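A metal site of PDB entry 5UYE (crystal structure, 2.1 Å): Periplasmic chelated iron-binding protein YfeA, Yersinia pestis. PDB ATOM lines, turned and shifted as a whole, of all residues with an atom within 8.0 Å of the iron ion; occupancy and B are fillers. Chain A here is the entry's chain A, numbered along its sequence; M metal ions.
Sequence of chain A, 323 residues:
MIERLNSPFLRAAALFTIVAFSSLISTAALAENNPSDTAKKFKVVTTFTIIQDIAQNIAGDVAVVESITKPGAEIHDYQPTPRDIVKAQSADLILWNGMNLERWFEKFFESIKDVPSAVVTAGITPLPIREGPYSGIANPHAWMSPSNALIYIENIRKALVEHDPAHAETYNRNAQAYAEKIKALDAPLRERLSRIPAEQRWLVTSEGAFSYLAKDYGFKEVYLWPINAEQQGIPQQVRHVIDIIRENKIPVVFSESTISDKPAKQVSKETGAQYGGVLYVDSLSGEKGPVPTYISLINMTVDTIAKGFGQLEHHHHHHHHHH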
ATOM      1  N   PHE A  48       7.261  22.180  -1.879  1.00  0.00           N
ATOM      2  CA  PHE A  48       7.922  20.937  -1.489  1.00  0.00           C
ATOM      3  C   PHE A  48       7.667  20.644  -0.011  1.00  0.00           C
ATOM      4  O   PHE A  48       7.042  21.422   0.719  1.00  0.00           O
ATOM      5  CB  PHE A  48       9.425  20.965  -1.846  1.00  0.00           C
ATOM      6  CG  PHE A  48      10.287  21.849  -0.958  1.00  0.00           C
ATOM      7  CD1 PHE A  48      10.111  23.224  -0.928  1.00  0.00           C
ATOM      8  CD2 PHE A  48      11.309  21.293  -0.195  1.00  0.00           C
ATOM      9  CE1 PHE A  48      10.915  24.042  -0.141  1.00  0.00           C
ATOM     10  CE2 PHE A  48      12.126  22.097   0.593  1.00  0.00           C
ATOM     11  CZ  PHE A  48      11.921  23.471   0.629  1.00  0.00           C
ATOM     12  N   GLU A  74      13.099  14.963  -6.631  1.00  0.00           N
ATOM     13  CA  GLU A  74      14.073  16.032  -6.791  1.00  0.00           C
ATOM     14  C   GLU A  74      13.339  17.356  -7.056  1.00  0.00           C
ATOM     15  O   GLU A  74      12.556  17.457  -8.005  1.00  0.00           O
ATOM     16  CB  GLU A  74      15.031  15.698  -7.929  1.00  0.00           C
ATOM     17  CG  GLU A  74      16.369  16.427  -7.888  1.00  0.00           C
ATOM     18  CD  GLU A  74      16.217  17.900  -8.205  1.00  0.00           C
ATOM     19  OE1 GLU A  74      15.868  18.244  -9.354  1.00  0.00           O
ATOM     20  OE2 GLU A  74      16.432  18.708  -7.302  1.00  0.00           O
ATOM     21  N   ILE A  75      13.605  18.358  -6.229  1.00  0.00           N
ATOM     22  CA  ILE A  75      12.770  19.558  -6.211  1.00  0.00           C
ATOM     23  C   ILE A  75      13.303  20.705  -7.069  1.00  0.00           C
ATOM     24  O   ILE A  75      12.514  21.576  -7.472  1.00  0.00           O
ATOM     25  CB  ILE A  75      12.571  20.052  -4.764  1.00  0.00           C
ATOM     26  CG1 ILE A  75      13.877  20.595  -4.178  1.00  0.00           C
ATOM     27  CG2 ILE A  75      12.042  18.925  -3.885  1.00  0.00           C
ATOM     28  CD1 ILE A  75      13.742  21.058  -2.683  1.00  0.00           C
ATOM     29  N   HIS A  76      14.609  20.747  -7.353  1.00  0.00           N
ATOM     30  CA  HIS A  76      15.163  21.902  -8.055  1.00  0.00           C
ATOM     31  C   HIS A  76      14.652  21.963  -9.502  1.00  0.00           C
ATOM     32  O   HIS A  76      14.167  23.009  -9.955  1.00  0.00           O
ATOM     33  CB  HIS A  76      16.689  21.836  -8.039  1.00  0.00           C
ATOM     34  CG  HIS A  76      17.310  21.982  -6.679  1.00  0.00           C
ATOM     35  ND1 HIS A  76      17.962  23.130  -6.275  1.00  0.00           N
ATOM     36  CD2 HIS A  76      17.407  21.108  -5.638  1.00  0.00           C
ATOM     37  CE1 HIS A  76      18.432  22.965  -5.050  1.00  0.00           C
ATOM     38  NE2 HIS A  76      18.112  21.756  -4.640  1.00  0.00           N
ATOM     39  N   LEU A 101      15.384  28.241  -5.554  1.00  0.00           N
ATOM     40  CA  LEU A 101      15.215  26.811  -5.332  1.00  0.00           C
ATOM     41  C   LEU A 101      14.448  26.199  -6.490  1.00  0.00           C
ATOM     42  O   LEU A 101      15.005  25.395  -7.250  1.00  0.00           O
ATOM     43  CB  LEU A 101      14.503  26.524  -4.001  1.00  0.00           C
ATOM     44  CG  LEU A 101      14.271  25.029  -3.700  1.00  0.00           C
ATOM     45  CD1 LEU A 101      15.581  24.236  -3.481  1.00  0.00           C
ATOM     46  CD2 LEU A 101      13.344  24.871  -2.496  1.00  0.00           C
ATOM     47  N   ASN A 139      22.264  30.596  -2.378  1.00  0.00           N
ATOM     48  CA  ASN A 139      22.033  29.185  -2.073  1.00  0.00           C
ATOM     49  C   ASN A 139      20.626  29.033  -1.505  1.00  0.00           C
ATOM     50  O   ASN A 139      20.302  29.682  -0.504  1.00  0.00           O
ATOM     51  CB  ASN A 139      23.110  28.717  -1.087  1.00  0.00           C
ATOM     52  CG  ASN A 139      23.093  27.213  -0.836  1.00  0.00           C
ATOM     53  OD1 ASN A 139      22.022  26.616  -0.732  1.00  0.00           O
ATOM     54  ND2 ASN A 139      24.277  26.610  -0.709  1.00  0.00           N
ATOM     55  N   PRO A 140      19.758  28.200  -2.099  1.00  0.00           N
ATOM     56  CA  PRO A 140      18.360  28.144  -1.627  1.00  0.00           C
ATOM     57  C   PRO A 140      18.140  27.412  -0.303  1.00  0.00           C
ATOM     58  O   PRO A 140      17.065  27.566   0.286  1.00  0.00           O
ATOM     59  CB  PRO A 140      17.649  27.395  -2.751  1.00  0.00           C
ATOM     60  CG  PRO A 140      18.716  26.475  -3.291  1.00  0.00           C
ATOM     61  CD  PRO A 140      19.975  27.334  -3.276  1.00  0.00           C
ATOM     62  N   HIS A 141      19.111  26.627   0.181  1.00  0.00           N
ATOM     63  CA  HIS A 141      18.864  25.679   1.260  1.00  0.00           C
ATOM     64  C   HIS A 141      18.910  26.342   2.628  1.00  0.00           C
ATOM     65  O   HIS A 141      19.545  25.820   3.548  1.00  0.00           O
ATOM     66  CB  HIS A 141      19.884  24.541   1.210  1.00  0.00           C
ATOM     67  CG  HIS A 141      19.877  23.782  -0.085  1.00  0.00           C
ATOM     68  ND1 HIS A 141      20.713  24.104  -1.134  1.00  0.00           N
ATOM     69  CD2 HIS A 141      19.096  22.771  -0.512  1.00  0.00           C
ATOM     70  CE1 HIS A 141      20.470  23.287  -2.143  1.00  0.00           C
ATOM     71  NE2 HIS A 141      19.495  22.458  -1.792  1.00  0.00           N
ATOM     72  N   TRP A 143      16.754  26.579   4.974  1.00  0.00           N
ATOM     73  CA  TRP A 143      16.053  25.906   6.069  1.00  0.00           C
ATOM     74  C   TRP A 143      16.925  24.946   6.875  1.00  0.00           C
ATOM     75  O   TRP A 143      16.464  24.469   7.921  1.00  0.00           O
ATOM     76  CB  TRP A 143      14.844  25.111   5.518  1.00  0.00           C
ATOM     77  CG  TRP A 143      15.232  24.028   4.560  1.00  0.00           C
ATOM     78  CD1 TRP A 143      15.611  22.743   4.866  1.00  0.00           C
ATOM     79  CD2 TRP A 143      15.297  24.130   3.127  1.00  0.00           C
ATOM     80  NE1 TRP A 143      15.898  22.044   3.717  1.00  0.00           N
ATOM     81  CE2 TRP A 143      15.728  22.871   2.634  1.00  0.00           C
ATOM     82  CE3 TRP A 143      15.051  25.163   2.213  1.00  0.00           C
ATOM     83  CZ2 TRP A 143      15.898  22.621   1.273  1.00  0.00           C
ATOM     84  CZ3 TRP A 143      15.213  24.907   0.851  1.00  0.00           C
ATOM     85  CH2 TRP A 143      15.624  23.647   0.394  1.00  0.00           C
ATOM     86  N   GLU A 207      25.395  17.143  -3.182  1.00  0.00           N
ATOM     87  CA  GLU A 207      25.025  18.526  -3.443  1.00  0.00           C
ATOM     88  C   GLU A 207      25.600  19.419  -2.343  1.00  0.00           C
ATOM     89  O   GLU A 207      25.637  19.029  -1.170  1.00  0.00           O
ATOM     90  CB  GLU A 207      23.503  18.700  -3.516  1.00  0.00           C
ATOM     91  CG  GLU A 207      23.083  20.155  -3.811  1.00  0.00           C
ATOM     92  CD  GLU A 207      21.574  20.394  -3.919  1.00  0.00           C
ATOM     93  OE1 GLU A 207      20.772  19.753  -3.202  1.00  0.00           O
ATOM     94  OE2 GLU A 207      21.196  21.255  -4.739  1.00  0.00           O
ATOM     95  N   GLY A 208      26.029  20.625  -2.718  1.00  0.00           N
ATOM     96  CA  GLY A 208      26.415  21.646  -1.731  1.00  0.00           C
ATOM     97  C   GLY A 208      25.205  22.250  -1.033  1.00  0.00           C
ATOM     98  O   GLY A 208      25.027  23.469  -1.009  1.00  0.00           O
ATOM     99  N   ALA A 209      24.369  21.396  -0.460  1.00  0.00           N
ATOM    100  CA  ALA A 209      23.089  21.780   0.098  1.00  0.00           C
ATOM    101  C   ALA A 209      23.171  22.170   1.561  1.00  0.00           C
ATOM    102  O   ALA A 209      22.159  22.564   2.148  1.00  0.00           O
ATOM    103  CB  ALA A 209      22.081  20.634  -0.064  1.00  0.00           C
ATOM    104  N   PHE A 210      24.345  22.077   2.183  1.00  0.00           N
ATOM    105  CA  PHE A 210      24.411  22.199   3.623  1.00  0.00           C
ATOM    106  C   PHE A 210      25.115  23.472   4.080  1.00  0.00           C
ATOM    107  O   PHE A 210      25.448  23.602   5.256  1.00  0.00           O
ATOM    108  CB  PHE A 210      25.066  20.941   4.204  1.00  0.00           C
ATOM    109  CG  PHE A 210      24.295  19.685   3.870  1.00  0.00           C
ATOM    110  CD1 PHE A 210      23.247  19.248   4.681  1.00  0.00           C
ATOM    111  CD2 PHE A 210      24.550  18.981   2.695  1.00  0.00           C
ATOM    112  CE1 PHE A 210      22.499  18.126   4.355  1.00  0.00           C
ATOM    113  CE2 PHE A 210      23.821  17.851   2.382  1.00  0.00           C
ATOM    114  CZ  PHE A 210      22.786  17.428   3.206  1.00  0.00           C
ATOM    115  N   TRP A 225      28.844  18.644  -6.222  1.00  0.00           N
ATOM    116  CA  TRP A 225      28.334  19.675  -7.144  1.00  0.00           C
ATOM    117  C   TRP A 225      27.630  20.784  -6.362  1.00  0.00           C
ATOM    118  O   TRP A 225      26.990  20.509  -5.334  1.00  0.00           O
ATOM    119  CB  TRP A 225      27.380  19.075  -8.197  1.00  0.00           C
ATOM    120  CG  TRP A 225      26.201  18.305  -7.660  1.00  0.00           C
ATOM    121  CD1 TRP A 225      24.971  18.797  -7.334  1.00  0.00           C
ATOM    122  CD2 TRP A 225      26.140  16.881  -7.443  1.00  0.00           C
ATOM    123  NE1 TRP A 225      24.152  17.779  -6.907  1.00  0.00           N
ATOM    124  CE2 TRP A 225      24.836  16.597  -6.966  1.00  0.00           C
ATOM    125  CE3 TRP A 225      27.041  15.827  -7.598  1.00  0.00           C
ATOM    126  CZ2 TRP A 225      24.420  15.301  -6.644  1.00  0.00           C
ATOM    127  CZ3 TRP A 225      26.633  14.538  -7.284  1.00  0.00           C
ATOM    128  CH2 TRP A 225      25.337  14.289  -6.804  1.00  0.00           C
ATOM    129  N   PRO A 226      27.741  22.040  -6.801  1.00  0.00           N
ATOM    130  CA  PRO A 226      27.277  23.165  -5.954  1.00  0.00           C
ATOM    131  C   PRO A 226      25.769  23.213  -5.746  1.00  0.00           C
ATOM    132  O   PRO A 226      25.319  23.570  -4.654  1.00  0.00           O
ATOM    133  CB  PRO A 226      27.786  24.412  -6.679  1.00  0.00           C
ATOM    134  CG  PRO A 226      28.149  23.956  -8.071  1.00  0.00           C
ATOM    135  CD  PRO A 226      28.518  22.502  -7.964  1.00  0.00           C
ATOM    136  N   ILE A 227      24.977  22.842  -6.745  1.00  0.00           N
ATOM    137  CA  ILE A 227      23.525  22.810  -6.644  1.00  0.00           C
ATOM    138  C   ILE A 227      23.014  21.828  -7.698  1.00  0.00           C
ATOM    139  O   ILE A 227      23.603  21.703  -8.780  1.00  0.00           O
ATOM    140  CB  ILE A 227      22.916  24.235  -6.827  1.00  0.00           C
ATOM    141  CG1 ILE A 227      21.406  24.227  -6.611  1.00  0.00           C
ATOM    142  CG2 ILE A 227      23.256  24.784  -8.211  1.00  0.00           C
ATOM    143  CD1 ILE A 227      20.846  25.614  -6.242  1.00  0.00           C
ATOM    144  N   ASN A 228      21.963  21.093  -7.354  1.00  0.00           N
ATOM    145  CA  ASN A 228      21.354  20.194  -8.318  1.00  0.00           C
ATOM    146  C   ASN A 228      21.064  20.940  -9.614  1.00  0.00           C
ATOM    147  O   ASN A 228      20.493  22.031  -9.613  1.00  0.00           O
ATOM    148  CB  ASN A 228      20.065  19.601  -7.740  1.00  0.00           C
ATOM    149  CG  ASN A 228      20.319  18.684  -6.557  1.00  0.00           C
ATOM    150  OD1 ASN A 228      21.458  18.453  -6.168  1.00  0.00           O
ATOM    151  ND2 ASN A 228      19.252  18.165  -5.974  1.00  0.00           N
ATOM    152  N   GLU A 256      22.597  12.443  -0.359  1.00  0.00           N
ATOM    153  CA  GLU A 256      21.329  13.009   0.087  1.00  0.00           C
ATOM    154  C   GLU A 256      20.169  12.252  -0.547  1.00  0.00           C
ATOM    155  O   GLU A 256      20.324  11.579  -1.573  1.00  0.00           O
ATOM    156  CB  GLU A 256      21.243  14.503  -0.240  1.00  0.00           C
ATOM    157  CG  GLU A 256      22.394  15.326   0.324  1.00  0.00           C
ATOM    158  CD  GLU A 256      23.583  15.384  -0.634  1.00  0.00           C
ATOM    159  OE1 GLU A 256      23.404  15.819  -1.805  1.00  0.00           O
ATOM    160  OE2 GLU A 256      24.697  14.976  -0.236  1.00  0.00           O
ATOM    161  N   THR A 258      17.335  12.733  -2.233  1.00  0.00           N
ATOM    162  CA  THR A 258      16.676  12.862  -3.537  1.00  0.00           C
ATOM    163  C   THR A 258      17.629  12.700  -4.720  1.00  0.00           C
ATOM    164  O   THR A 258      17.191  12.861  -5.869  1.00  0.00           O
ATOM    165  CB  THR A 258      15.944  14.202  -3.671  1.00  0.00           C
ATOM    166  OG1 THR A 258      16.888  15.284  -3.824  1.00  0.00           O
ATOM    167  CG2 THR A 258      15.032  14.447  -2.468  1.00  0.00           C
ATOM    168  N   ILE A 259      18.898  12.410  -4.497  1.00  0.00           N
ATOM    169  CA  ILE A 259      19.866  12.272  -5.576  1.00  0.00           C
ATOM    170  C   ILE A 259      20.559  10.910  -5.429  1.00  0.00           C
ATOM    171  O   ILE A 259      20.322  10.166  -4.482  1.00  0.00           O
ATOM    172  CB  ILE A 259      20.886  13.439  -5.593  1.00  0.00           C
ATOM    173  CG1 ILE A 259      21.484  13.704  -4.201  1.00  0.00           C
ATOM    174  CG2 ILE A 259      20.204  14.709  -6.086  1.00  0.00           C
ATOM    175  CD1 ILE A 259      22.713  12.831  -3.886  1.00  0.00           C
ATOM    176  N   VAL A 281      17.715  16.682   3.179  1.00  0.00           N
ATOM    177  CA  VAL A 281      17.744  18.138   3.039  1.00  0.00           C
ATOM    178  C   VAL A 281      16.648  18.619   2.090  1.00  0.00           C
ATOM    179  O   VAL A 281      15.881  19.529   2.430  1.00  0.00           O
ATOM    180  CB  VAL A 281      19.141  18.639   2.594  1.00  0.00           C
ATOM    181  CG1 VAL A 281      19.693  17.855   1.379  1.00  0.00           C
ATOM    182  CG2 VAL A 281      19.092  20.146   2.304  1.00  0.00           C
ATOM    183  N   ASP A 282      16.526  18.012   0.916  1.00  0.00           N
ATOM    184  CA  ASP A 282      15.563  18.535  -0.063  1.00  0.00           C
ATOM    185  C   ASP A 282      14.171  17.912   0.085  1.00  0.00           C
ATOM    186  O   ASP A 282      13.217  18.440  -0.508  1.00  0.00           O
ATOM    187  CB  ASP A 282      16.072  18.298  -1.495  1.00  0.00           C
ATOM    188  CG  ASP A 282      17.161  19.312  -1.913  1.00  0.00           C
ATOM    189  OD1 ASP A 282      17.480  20.222  -1.122  1.00  0.00           O
ATOM    190  OD2 ASP A 282      17.690  19.196  -3.024  1.00  0.00           O
ATOM    191  N   SER A 283      14.041  16.821   0.831  1.00  0.00           N
ATOM    192  CA  SER A 283      12.736  16.188   1.021  1.00  0.00           C
ATOM    193  C   SER A 283      12.660  15.529   2.389  1.00  0.00           C
ATOM    194  O   SER A 283      13.655  15.005   2.896  1.00  0.00           O
ATOM    195  CB  SER A 283      12.450  15.141  -0.074  1.00  0.00           C
ATOM    196  OG  SER A 283      11.138  14.595   0.077  1.00  0.00           O
HETATM  197 FE    FE M   1      19.003  20.849  -3.071  1.00  0.00          FE
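The iron ion is bound by NE2 of His 76 (2.0 Å), OE1 of Glu 207 (2.1 Å), OD2 of Asp 282 (2.1 Å), NE2 of His 141 (2.1 Å) and OD1 of Asp 282 (2.6 Å). Slightly farther from the iron ion lies the side-chain carboxylate (OE2) of Glu 207 (2.8 Å).
OE2 of Glu 74 is in hydrogen-bond range of N of His 76 (2.7 Å). N of Asn 228 sits at hydrogen-bond distance from OE2 of Glu 207, at 2.7 Å. The side-chain carboxylate (OE1) of Glu 256 sits at hydrogen-bond distance from the backbone NH (N) of Glu 207, 2.8 Å away. The side-chain carboxylate (OD2) of Asp 282 lies close to the side-chain amide nitrogen (ND2) of Asn 228. A ring nitrogen (ND1) of His 141 is in hydrogen-bond range of the side-chain amide oxygen (OD1) of Asn 139, 2.9 Å away. OE2 of Glu 74 is in hydrogen-bond range of ND2 of Asn 228 (3.2 Å). The side-chain amide oxygen of Asn 228 is in hydrogen-bond range of the indole nitrogen of Trp 225 (2.9 Å).
Merely in contact with the iron ion: Asn 228 (3.96 Å). Five residues have an atom within 4 Å of the iron ion: His 76, His 141, Glu 207, Asn 228 and Asp 282.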
